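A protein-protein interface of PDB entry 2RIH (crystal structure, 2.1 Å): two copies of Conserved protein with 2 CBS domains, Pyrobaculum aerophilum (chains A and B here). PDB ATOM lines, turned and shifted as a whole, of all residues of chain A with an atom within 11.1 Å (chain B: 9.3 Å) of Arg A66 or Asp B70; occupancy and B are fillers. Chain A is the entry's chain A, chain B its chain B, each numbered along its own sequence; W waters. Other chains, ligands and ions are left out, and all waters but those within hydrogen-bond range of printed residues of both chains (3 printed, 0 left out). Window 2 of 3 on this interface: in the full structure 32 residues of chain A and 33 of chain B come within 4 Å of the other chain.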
ATOM      1  N   ILE A  24     -19.461  18.278  20.653  1.00  0.00           N
ATOM      2  CA  ILE A  24     -18.513  18.106  21.745  1.00  0.00           C
ATOM      3  C   ILE A  24     -18.745  19.116  22.871  1.00  0.00           C
ATOM      4  O   ILE A  24     -18.695  18.755  24.045  1.00  0.00           O
ATOM      5  CB  ILE A  24     -17.044  18.215  21.251  1.00  0.00           C
ATOM      6  CG1 ILE A  24     -16.719  17.066  20.281  1.00  0.00           C
ATOM      7  CG2 ILE A  24     -16.084  18.233  22.457  1.00  0.00           C
ATOM      8  CD1 ILE A  24     -15.411  17.227  19.585  1.00  0.00           C
ATOM      9  N   ARG A  25     -18.979  20.374  22.514  1.00  0.00           N
ATOM     10  CA  ARG A  25     -19.199  21.416  23.516  1.00  0.00           C
ATOM     11  C   ARG A  25     -20.547  21.269  24.223  1.00  0.00           C
ATOM     12  O   ARG A  25     -20.675  21.660  25.384  1.00  0.00           O
ATOM     13  CB  ARG A  25     -19.092  22.822  22.902  1.00  0.00           C
ATOM     14  CG  ARG A  25     -18.774  23.894  23.951  1.00  0.00           C
ATOM     15  CD  ARG A  25     -18.606  25.277  23.365  1.00  0.00           C
ATOM     16  NE  ARG A  25     -17.702  25.314  22.217  1.00  0.00           N
ATOM     17  CZ  ARG A  25     -16.381  25.501  22.257  1.00  0.00           C
ATOM     18  NH1 ARG A  25     -15.737  25.664  23.404  1.00  0.00           N
ATOM     19  NH2 ARG A  25     -15.691  25.525  21.125  1.00  0.00           N
ATOM     20  N   ASP A  58     -12.227  12.147  27.162  1.00  0.00           N
ATOM     21  CA  ASP A  58     -12.331  12.226  25.706  1.00  0.00           C
ATOM     22  C   ASP A  58     -12.291  13.685  25.251  1.00  0.00           C
ATOM     23  O   ASP A  58     -11.678  14.020  24.236  1.00  0.00           O
ATOM     24  CB  ASP A  58     -13.615  11.550  25.218  1.00  0.00           C
ATOM     25  CG  ASP A  58     -13.653  10.061  25.542  1.00  0.00           C
ATOM     26  OD1 ASP A  58     -12.692   9.328  25.197  1.00  0.00           O
ATOM     27  OD2 ASP A  58     -14.654   9.625  26.137  1.00  0.00           O
ATOM     28  N   ILE A  59     -12.956  14.548  26.009  1.00  0.00           N
ATOM     29  CA  ILE A  59     -12.935  15.984  25.745  1.00  0.00           C
ATOM     30  C   ILE A  59     -11.513  16.542  25.923  1.00  0.00           C
ATOM     31  O   ILE A  59     -11.069  17.398  25.147  1.00  0.00           O
ATOM     32  CB  ILE A  59     -13.966  16.705  26.644  1.00  0.00           C
ATOM     33  CG1 ILE A  59     -15.385  16.336  26.172  1.00  0.00           C
ATOM     34  CG2 ILE A  59     -13.732  18.233  26.639  1.00  0.00           C
ATOM     35  CD1 ILE A  59     -16.487  16.563  27.188  1.00  0.00           C
ATOM     36  N   LEU A  60     -10.804  16.045  26.938  1.00  0.00           N
ATOM     37  CA  LEU A  60      -9.420  16.425  27.184  1.00  0.00           C
ATOM     38  C   LEU A  60      -8.567  16.150  25.937  1.00  0.00           C
ATOM     39  O   LEU A  60      -7.805  17.009  25.489  1.00  0.00           O
ATOM     40  CB  LEU A  60      -8.870  15.634  28.384  1.00  0.00           C
ATOM     41  CG  LEU A  60      -7.476  15.953  28.920  1.00  0.00           C
ATOM     42  CD1 LEU A  60      -7.528  17.189  29.793  1.00  0.00           C
ATOM     43  CD2 LEU A  60      -6.922  14.770  29.733  1.00  0.00           C
ATOM     44  N   ARG A  61      -8.701  14.938  25.399  1.00  0.00           N
ATOM     45  CA  ARG A  61      -7.971  14.534  24.195  1.00  0.00           C
ATOM     46  C   ARG A  61      -8.334  15.416  22.998  1.00  0.00           C
ATOM     47  O   ARG A  61      -7.469  15.762  22.185  1.00  0.00           O
ATOM     48  CB  ARG A  61      -8.241  13.059  23.874  1.00  0.00           C
ATOM     49  CG  ARG A  61      -7.617  12.582  22.562  1.00  0.00           C
ATOM     50  CD  ARG A  61      -7.888  11.102  22.290  1.00  0.00           C
ATOM     51  NE  ARG A  61      -9.290  10.748  22.498  1.00  0.00           N
ATOM     52  CZ  ARG A  61     -10.290  11.051  21.673  1.00  0.00           C
ATOM     53  NH1 ARG A  61     -11.524  10.671  21.986  1.00  0.00           N
ATOM     54  NH2 ARG A  61     -10.076  11.732  20.547  1.00  0.00           N
ATOM     55  N   ALA A  62      -9.613  15.779  22.898  1.00  0.00           N
ATOM     56  CA  ALA A  62     -10.117  16.660  21.845  1.00  0.00           C
ATOM     57  C   ALA A  62      -9.421  18.017  21.875  1.00  0.00           C
ATOM     58  O   ALA A  62      -9.018  18.537  20.838  1.00  0.00           O
ATOM     59  CB  ALA A  62     -11.633  16.845  21.996  1.00  0.00           C
ATOM     60  N   VAL A  63      -9.297  18.577  23.074  1.00  0.00           N
ATOM     61  CA  VAL A  63      -8.590  19.828  23.314  1.00  0.00           C
ATOM     62  C   VAL A  63      -7.112  19.701  22.890  1.00  0.00           C
ATOM     63  O   VAL A  63      -6.617  20.518  22.126  1.00  0.00           O
ATOM     64  CB  VAL A  63      -8.688  20.233  24.816  1.00  0.00           C
ATOM     65  CG1 VAL A  63      -7.780  21.416  25.141  1.00  0.00           C
ATOM     66  CG2 VAL A  63     -10.129  20.548  25.197  1.00  0.00           C
ATOM     67  N   ALA A  64      -6.435  18.662  23.381  1.00  0.00           N
ATOM     68  CA  ALA A  64      -5.026  18.393  23.055  1.00  0.00           C
ATOM     69  C   ALA A  64      -4.777  18.303  21.547  1.00  0.00           C
ATOM     70  O   ALA A  64      -3.735  18.752  21.061  1.00  0.00           O
ATOM     71  CB  ALA A  64      -4.547  17.094  23.754  1.00  0.00           C
ATOM     72  N   GLN A  65      -5.745  17.746  20.818  1.00  0.00           N
ATOM     73  CA  GLN A  65      -5.643  17.560  19.369  1.00  0.00           C
ATOM     74  C   GLN A  65      -6.176  18.738  18.550  1.00  0.00           C
ATOM     75  O   GLN A  65      -6.131  18.707  17.323  1.00  0.00           O
ATOM     76  CB  GLN A  65      -6.366  16.278  18.957  1.00  0.00           C
ATOM     77  CG  GLN A  65      -5.677  15.008  19.451  1.00  0.00           C
ATOM     78  CD  GLN A  65      -6.483  13.753  19.180  1.00  0.00           C
ATOM     79  OE1 GLN A  65      -7.596  13.814  18.661  1.00  0.00           O
ATOM     80  NE2 GLN A  65      -5.928  12.605  19.542  1.00  0.00           N
ATOM     81  N   ARG A  66      -6.670  19.772  19.227  1.00  0.00           N
ATOM     82  CA  ARG A  66      -7.175  20.985  18.573  1.00  0.00           C
ATOM     83  C   ARG A  66      -8.337  20.702  17.618  1.00  0.00           C
ATOM     84  O   ARG A  66      -8.438  21.297  16.548  1.00  0.00           O
ATOM     85  CB  ARG A  66      -6.046  21.720  17.842  1.00  0.00           C
ATOM     86  CG  ARG A  66      -4.798  21.918  18.681  1.00  0.00           C
ATOM     87  CD  ARG A  66      -3.780  22.796  17.976  1.00  0.00           C
ATOM     88  NE  ARG A  66      -4.158  24.197  18.094  1.00  0.00           N
ATOM     89  CZ  ARG A  66      -3.560  25.109  18.860  1.00  0.00           C
ATOM     90  NH1 ARG A  66      -2.490  24.827  19.599  1.00  0.00           N
ATOM     91  NH2 ARG A  66      -4.048  26.339  18.875  1.00  0.00           N
ATOM     92  N   LEU A  67      -9.215  19.789  18.020  1.00  0.00           N
ATOM     93  CA  LEU A  67     -10.410  19.491  17.247  1.00  0.00           C
ATOM     94  C   LEU A  67     -11.403  20.637  17.342  1.00  0.00           C
ATOM     95  O   LEU A  67     -11.392  21.433  18.300  1.00  0.00           O
ATOM     96  CB  LEU A  67     -11.092  18.220  17.748  1.00  0.00           C
ATOM     97  CG  LEU A  67     -10.297  16.917  17.793  1.00  0.00           C
ATOM     98  CD1 LEU A  67     -11.235  15.774  18.191  1.00  0.00           C
ATOM     99  CD2 LEU A  67      -9.606  16.637  16.457  1.00  0.00           C
ATOM    100  N   ASP A  68     -12.263  20.712  16.337  1.00  0.00           N
ATOM    101  CA  ASP A  68     -13.378  21.626  16.359  1.00  0.00           C
ATOM    102  C   ASP A  68     -14.325  21.133  17.455  1.00  0.00           C
ATOM    103  O   ASP A  68     -15.049  20.150  17.277  1.00  0.00           O
ATOM    104  CB  ASP A  68     -14.065  21.660  14.991  1.00  0.00           C
ATOM    105  CG  ASP A  68     -15.182  22.685  14.915  1.00  0.00           C
ATOM    106  OD1 ASP A  68     -15.727  22.850  13.807  1.00  0.00           O
ATOM    107  OD2 ASP A  68     -15.515  23.333  15.937  1.00  0.00           O
ATOM    108  N   LEU A  69     -14.291  21.828  18.588  1.00  0.00           N
ATOM    109  CA  LEU A  69     -15.096  21.491  19.771  1.00  0.00           C
ATOM    110  C   LEU A  69     -16.597  21.750  19.573  1.00  0.00           C
ATOM    111  O   LEU A  69     -17.416  21.336  20.386  1.00  0.00           O
ATOM    112  CB  LEU A  69     -14.569  22.258  20.990  1.00  0.00           C
ATOM    113  CG  LEU A  69     -13.450  21.657  21.865  1.00  0.00           C
ATOM    114  CD1 LEU A  69     -12.596  20.612  21.180  1.00  0.00           C
ATOM    115  CD2 LEU A  69     -12.591  22.788  22.457  1.00  0.00           C
ATOM    116  N   ASP A  70     -16.954  22.440  18.495  1.00  0.00           N
ATOM    117  CA  ASP A  70     -18.357  22.581  18.096  1.00  0.00           C
ATOM    118  C   ASP A  70     -18.740  21.608  16.976  1.00  0.00           C
ATOM    119  O   ASP A  70     -19.819  21.709  16.404  1.00  0.00           O
ATOM    120  CB  ASP A  70     -18.644  24.022  17.686  1.00  0.00           C
ATOM    121  CG  ASP A  70     -18.577  24.968  18.853  1.00  0.00           C
ATOM    122  OD1 ASP A  70     -19.367  24.799  19.797  1.00  0.00           O
ATOM    123  OD2 ASP A  70     -17.728  25.871  18.830  1.00  0.00           O
ATOM    124  N   GLY A  71     -17.852  20.669  16.674  1.00  0.00           N
ATOM    125  CA  GLY A  71     -18.164  19.561  15.781  1.00  0.00           C
ATOM    126  C   GLY A  71     -18.827  18.425  16.557  1.00  0.00           C
ATOM    127  O   GLY A  71     -18.985  18.503  17.778  1.00  0.00           O
ATOM    128  N   PRO A  72     -19.237  17.362  15.850  1.00  0.00           N
ATOM    129  CA  PRO A  72     -19.899  16.234  16.494  1.00  0.00           C
ATOM    130  C   PRO A  72     -19.068  15.540  17.581  1.00  0.00           C
ATOM    131  O   PRO A  72     -17.838  15.415  17.454  1.00  0.00           O
ATOM    132  CB  PRO A  72     -20.179  15.277  15.326  1.00  0.00           C
ATOM    133  CG  PRO A  72     -19.267  15.694  14.244  1.00  0.00           C
ATOM    134  CD  PRO A  72     -19.113  17.168  14.394  1.00  0.00           C
ATOM    135  N   ILE A  76     -15.593  11.226  18.844  1.00  0.00           N
ATOM    136  CA  ILE A  76     -14.688  11.096  19.995  1.00  0.00           C
ATOM    137  C   ILE A  76     -15.244  10.132  21.055  1.00  0.00           C
ATOM    138  O   ILE A  76     -14.602   9.886  22.074  1.00  0.00           O
ATOM    139  CB  ILE A  76     -14.321  12.464  20.624  1.00  0.00           C
ATOM    140  CG1 ILE A  76     -15.492  13.092  21.387  1.00  0.00           C
ATOM    141  CG2 ILE A  76     -13.813  13.407  19.549  1.00  0.00           C
ATOM    142  CD1 ILE A  76     -15.071  14.183  22.341  1.00  0.00           C
ATOM    143  N   THR B  21       3.366  28.962  34.025  1.00  0.00           N
ATOM    144  CA  THR B  21       3.104  29.691  32.789  1.00  0.00           C
ATOM    145  C   THR B  21       2.388  28.865  31.695  1.00  0.00           C
ATOM    146  O   THR B  21       2.100  29.375  30.614  1.00  0.00           O
ATOM    147  CB  THR B  21       4.447  30.179  32.203  1.00  0.00           C
ATOM    148  OG1 THR B  21       5.400  29.115  32.273  1.00  0.00           O
ATOM    149  CG2 THR B  21       4.976  31.367  32.985  1.00  0.00           C
ATOM    150  N   ALA B  22       2.118  27.594  31.963  1.00  0.00           N
ATOM    151  CA  ALA B  22       1.486  26.708  30.983  1.00  0.00           C
ATOM    152  C   ALA B  22       0.131  27.230  30.503  1.00  0.00           C
ATOM    153  O   ALA B  22      -0.609  27.864  31.269  1.00  0.00           O
ATOM    154  CB  ALA B  22       1.322  25.316  31.571  1.00  0.00           C
ATOM    155  N   THR B  23      -0.165  26.982  29.227  1.00  0.00           N
ATOM    156  CA  THR B  23      -1.487  27.264  28.671  1.00  0.00           C
ATOM    157  C   THR B  23      -2.409  26.105  29.006  1.00  0.00           C
ATOM    158  O   THR B  23      -1.951  25.024  29.400  1.00  0.00           O
ATOM    159  CB  THR B  23      -1.470  27.461  27.140  1.00  0.00           C
ATOM    160  OG1 THR B  23      -1.137  26.227  26.484  1.00  0.00           O
ATOM    161  CG2 THR B  23      -0.476  28.564  26.731  1.00  0.00           C
ATOM    162  N   ILE B  24      -3.708  26.332  28.847  1.00  0.00           N
ATOM    163  CA  ILE B  24      -4.701  25.296  29.110  1.00  0.00           C
ATOM    164  C   ILE B  24      -4.461  24.077  28.204  1.00  0.00           C
ATOM    165  O   ILE B  24      -4.489  22.944  28.678  1.00  0.00           O
ATOM    166  CB  ILE B  24      -6.160  25.823  28.933  1.00  0.00           C
ATOM    167  CG1 ILE B  24      -6.439  27.009  29.866  1.00  0.00           C
ATOM    168  CG2 ILE B  24      -7.165  24.720  29.193  1.00  0.00           C
ATOM    169  CD1 ILE B  24      -7.804  27.626  29.694  1.00  0.00           C
ATOM    170  N   ARG B  25      -4.217  24.311  26.913  1.00  0.00           N
ATOM    171  CA  ARG B  25      -4.019  23.211  25.965  1.00  0.00           C
ATOM    172  C   ARG B  25      -2.736  22.421  26.217  1.00  0.00           C
ATOM    173  O   ARG B  25      -2.689  21.210  25.955  1.00  0.00           O
ATOM    174  CB  ARG B  25      -4.035  23.710  24.521  1.00  0.00           C
ATOM    175  CG  ARG B  25      -4.390  22.614  23.530  1.00  0.00           C
ATOM    176  CD  ARG B  25      -4.291  23.069  22.114  1.00  0.00           C
ATOM    177  NE  ARG B  25      -4.997  24.321  21.863  1.00  0.00           N
ATOM    178  CZ  ARG B  25      -6.312  24.444  21.685  1.00  0.00           C
ATOM    179  NH1 ARG B  25      -7.120  23.392  21.735  1.00  0.00           N
ATOM    180  NH2 ARG B  25      -6.828  25.640  21.450  1.00  0.00           N
ATOM    181  N   GLU B  26      -1.703  23.098  26.725  1.00  0.00           N
ATOM    182  CA  GLU B  26      -0.450  22.442  27.097  1.00  0.00           C
ATOM    183  C   GLU B  26      -0.666  21.448  28.218  1.00  0.00           C
ATOM    184  O   GLU B  26      -0.100  20.354  28.185  1.00  0.00           O
ATOM    185  CB  GLU B  26       0.623  23.455  27.507  1.00  0.00           C
ATOM    186  CG  GLU B  26       1.290  24.101  26.323  1.00  0.00           C
ATOM    187  CD  GLU B  26       2.082  25.346  26.668  1.00  0.00           C
ATOM    188  OE1 GLU B  26       2.129  25.768  27.846  1.00  0.00           O
ATOM    189  OE2 GLU B  26       2.670  25.891  25.728  1.00  0.00           O
ATOM    190  N   VAL B  27      -1.488  21.827  29.199  1.00  0.00           N
ATOM    191  CA  VAL B  27      -1.839  20.929  30.298  1.00  0.00           C
ATOM    192  C   VAL B  27      -2.636  19.736  29.767  1.00  0.00           C
ATOM    193  O   VAL B  27      -2.342  18.591  30.114  1.00  0.00           O
ATOM    194  CB  VAL B  27      -2.657  21.657  31.406  1.00  0.00           C
ATOM    195  CG1 VAL B  27      -3.116  20.663  32.487  1.00  0.00           C
ATOM    196  CG2 VAL B  27      -1.849  22.805  32.014  1.00  0.00           C
ATOM    197  N   ALA B  28      -3.637  20.015  28.928  1.00  0.00           N
ATOM    198  CA  ALA B  28      -4.448  18.970  28.289  1.00  0.00           C
ATOM    199  C   ALA B  28      -3.594  17.972  27.492  1.00  0.00           C
ATOM    200  O   ALA B  28      -3.824  16.763  27.558  1.00  0.00           O
ATOM    201  CB  ALA B  28      -5.536  19.593  27.396  1.00  0.00           C
ATOM    202  N   THR B  29      -2.608  18.477  26.760  1.00  0.00           N
ATOM    203  CA  THR B  29      -1.688  17.619  25.993  1.00  0.00           C
ATOM    204  C   THR B  29      -0.936  16.631  26.894  1.00  0.00           C
ATOM    205  O   THR B  29      -0.860  15.435  26.592  1.00  0.00           O
ATOM    206  CB  THR B  29      -0.671  18.472  25.202  1.00  0.00           C
ATOM    207  OG1 THR B  29      -1.367  19.257  24.231  1.00  0.00           O
ATOM    208  CG2 THR B  29       0.364  17.611  24.495  1.00  0.00           C
ATOM    209  N   ALA B  62     -13.672  24.866  31.181  1.00  0.00           N
ATOM    210  CA  ALA B  62     -13.133  25.881  30.252  1.00  0.00           C
ATOM    211  C   ALA B  62     -13.726  25.733  28.849  1.00  0.00           C
ATOM    212  O   ALA B  62     -14.043  26.730  28.197  1.00  0.00           O
ATOM    213  CB  ALA B  62     -11.620  25.797  30.186  1.00  0.00           C
ATOM    214  N   ARG B  66     -16.396  28.319  26.769  1.00  0.00           N
ATOM    215  CA  ARG B  66     -15.720  28.874  25.588  1.00  0.00           C
ATOM    216  C   ARG B  66     -14.526  29.768  25.904  1.00  0.00           C
ATOM    217  O   ARG B  66     -14.348  30.816  25.275  1.00  0.00           O
ATOM    218  CB  ARG B  66     -16.692  29.663  24.712  1.00  0.00           C
ATOM    219  CG  ARG B  66     -17.721  28.828  24.061  1.00  0.00           C
ATOM    220  CD  ARG B  66     -18.607  29.676  23.187  1.00  0.00           C
ATOM    221  NE  ARG B  66     -19.603  28.831  22.563  1.00  0.00           N
ATOM    222  CZ  ARG B  66     -19.435  28.171  21.422  1.00  0.00           C
ATOM    223  NH1 ARG B  66     -18.302  28.267  20.726  1.00  0.00           N
ATOM    224  NH2 ARG B  66     -20.429  27.417  20.966  1.00  0.00           N
ATOM    225  N   LEU B  67     -13.706  29.363  26.867  1.00  0.00           N
ATOM    226  CA  LEU B  67     -12.469  30.088  27.139  1.00  0.00           C
ATOM    227  C   LEU B  67     -11.495  29.833  25.996  1.00  0.00           C
ATOM    228  O   LEU B  67     -11.613  28.826  25.290  1.00  0.00           O
ATOM    229  CB  LEU B  67     -11.839  29.633  28.456  1.00  0.00           C
ATOM    230  CG  LEU B  67     -12.663  29.788  29.733  1.00  0.00           C
ATOM    231  CD1 LEU B  67     -11.771  29.477  30.927  1.00  0.00           C
ATOM    232  CD2 LEU B  67     -13.278  31.177  29.855  1.00  0.00           C
ATOM    233  N   ASP B  68     -10.555  30.756  25.805  1.00  0.00           N
ATOM    234  CA  ASP B  68      -9.439  30.555  24.883  1.00  0.00           C
ATOM    235  C   ASP B  68      -8.527  29.501  25.512  1.00  0.00           C
ATOM    236  O   ASP B  68      -7.891  29.752  26.537  1.00  0.00           O
ATOM    237  CB  ASP B  68      -8.677  31.867  24.662  1.00  0.00           C
ATOM    238  CG  ASP B  68      -7.533  31.737  23.660  1.00  0.00           C
ATOM    239  OD1 ASP B  68      -6.947  32.785  23.305  1.00  0.00           O
ATOM    240  OD2 ASP B  68      -7.227  30.609  23.217  1.00  0.00           O
ATOM    241  N   LEU B  69      -8.459  28.328  24.893  1.00  0.00           N
ATOM    242  CA  LEU B  69      -7.705  27.199  25.463  1.00  0.00           C
ATOM    243  C   LEU B  69      -6.196  27.342  25.244  1.00  0.00           C
ATOM    244  O   LEU B  69      -5.416  26.553  25.763  1.00  0.00           O
ATOM    245  CB  LEU B  69      -8.232  25.871  24.912  1.00  0.00           C
ATOM    246  CG  LEU B  69      -9.758  25.724  25.024  1.00  0.00           C
ATOM    247  CD1 LEU B  69     -10.247  24.444  24.347  1.00  0.00           C
ATOM    248  CD2 LEU B  69     -10.218  25.788  26.497  1.00  0.00           C
ATOM    249  N   ASP B  70      -5.795  28.353  24.476  1.00  0.00           N
ATOM    250  CA  ASP B  70      -4.387  28.729  24.354  1.00  0.00           C
ATOM    251  C   ASP B  70      -4.002  29.828  25.350  1.00  0.00           C
ATOM    252  O   ASP B  70      -2.843  30.225  25.421  1.00  0.00           O
ATOM    253  CB  ASP B  70      -4.076  29.129  22.914  1.00  0.00           C
ATOM    254  CG  ASP B  70      -4.194  27.956  21.972  1.00  0.00           C
ATOM    255  OD1 ASP B  70      -3.622  26.894  22.304  1.00  0.00           O
ATOM    256  OD2 ASP B  70      -4.884  28.074  20.935  1.00  0.00           O
ATOM    257  N   GLY B  71      -4.974  30.283  26.138  1.00  0.00           N
ATOM    258  CA  GLY B  71      -4.711  31.196  27.246  1.00  0.00           C
ATOM    259  C   GLY B  71      -4.116  30.442  28.424  1.00  0.00           C
ATOM    260  O   GLY B  71      -4.019  29.215  28.387  1.00  0.00           O
ATOM    261  N   PRO B  72      -3.720  31.172  29.483  1.00  0.00           N
ATOM    262  CA  PRO B  72      -3.038  30.584  30.634  1.00  0.00           C
ATOM    263  C   PRO B  72      -3.899  29.626  31.470  1.00  0.00           C
ATOM    264  O   PRO B  72      -5.086  29.871  31.666  1.00  0.00           O
ATOM    265  CB  PRO B  72      -2.627  31.814  31.462  1.00  0.00           C
ATOM    266  CG  PRO B  72      -3.586  32.857  31.083  1.00  0.00           C
ATOM    267  CD  PRO B  72      -3.901  32.628  29.641  1.00  0.00           C
ATOM    268  N   ALA B  73      -3.281  28.563  31.974  1.00  0.00           N
ATOM    269  CA  ALA B  73      -3.973  27.579  32.820  1.00  0.00           C
ATOM    270  C   ALA B  73      -4.159  28.028  34.277  1.00  0.00           C
ATOM    271  O   ALA B  73      -5.093  27.586  34.941  1.00  0.00           O
ATOM    272  CB  ALA B  73      -3.238  26.236  32.782  1.00  0.00           C
HETATM  273  O   HOH W   1     -13.097  26.794  24.478  1.00  0.00           O
HETATM  274  O   HOH W   2      -1.919  20.738  21.915  1.00  0.00           O
HETATM  275  O   HOH W   3      -9.829  22.151  20.636  1.00  0.00           O
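Asp B70 touches just one residue of chain A: Arg A66.
No residue of chain A comes within 4 Å of Thr B23.
Ile B24 touches none of the printed residues of chain A.
Of chain A, only Val A63 (2.9 Å) and Arg A66 (3.4 Å) come within 4 Å of Arg B25.
Printed residues of chain A within 4 Å of Leu B69: Val A63 and Leu A69.
Of the printed residues of chain B, Leu A69 touches Leu B69.
Printed residues of chain B within 4 Å of Ala A64: Ala B28 and Thr B29.
The nearest residue of chain A that does not touch Asp B70 is Val A63 (7.0 Å).
The nearest printed residue of chain B that does not touch Val A63 is Ile B24 (5.1 Å).
Hydrophobic or aromatic side chains of chain B that line the printed part of chain A: Ala B28 and Leu B69.
Along chain B the printed residues that touch a printed residue of chain A span positions 25 to 70.
Of the 18 printed residues of chain A, 7 touch a printed residue of chain B.
Hydrophobic or aromatic side chains of chain A within 4 Å of the printed part of chain B: Leu A60, Val A63, Ala A64 and Leu A69.
Among the printed residues, Asp or Glu carboxylates within 4 Å of a Lys or Arg side-chain nitrogen of the other chain: Arg A66 with Asp B70 and Asp A70 with Arg B66.
NE of Arg A25 lies within salt-bridge range of OD1 of Asp A70.
N of Arg A25 sits at hydrogen-bond distance from O of Leu A69, 2.8 Å away.
N of Arg B25 lies within hydrogen-bond range of O of Leu B69.
The backbone NH (N) of Asp B70 lies within hydrogen-bond range of the side-chain carboxylate (OD2) of Asp B68, 3.0 Å away.
OD2 of Asp A68 is in hydrogen-bond range of N of Asp A70 (3.1 Å).
The side-chain hydroxyl (OG1) of Thr B29 is in hydrogen-bond range of the backbone carbonyl oxygen (O) of Arg B25, 2.9 Å away.
CA of Ala B28 touches CD1 of Leu A60 (3.9 Å).
Val A63 touches Ala B28.
CG1 of Val A63 touches CD1 of Leu B69, at 3.99 Å.
Ala A64 touches Ala B28 (CB to O, 3.9 Å).
Thr B29 touches Ala A64 (CA to CB, 3.7 Å).
Leu A69 touches Leu B69.
Water W1 bridges O of Leu B67 (2.6 Å) and NH1 of Arg A25 (3.1 Å).
Water W2 bridges OG1 of Thr B29 (2.8 Å) and O of Ala A64 (2.8 Å).
Water W3 lies within hydrogen-bond range of O of Leu A67 (2.9 Å) and NH1 of Arg B25 (3.2 Å).
Arg A25 touches Arg B66, and with the chains exchanged Arg A66 touches Arg B25.
Arg A66 touches Asp B70, and with the chains exchanged Asp A70 touches Arg B66.
Leu A69 touches its own counterpart, Leu B69.
Positions printed for both chains: 24, 25, 62, 66, 67, 68, 69, 70, 71 and 72.
Of the 11 pairs that touch across the chains among the printed residues, 5 have their exchanged pair printed and touching as well.
The side-chain carboxylate (OD1) of Asp A70 is in salt-bridge range of the guanidinium group (NH2) of Arg B66 (3.1 Å).
NH2 of Arg A66 is in salt-bridge range of OD2 of Asp B70, at 2.8 Å.
The guanidinium group of Arg A25 lies close to the guanidinium group of Arg B66 (3.4 Å).
NE of Arg B25 sits close to NH1 of Arg A66, at 3.4 Å.
NH1 of Arg B25 sits at hydrogen-bond distance from O of Val A63 (2.9 Å).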
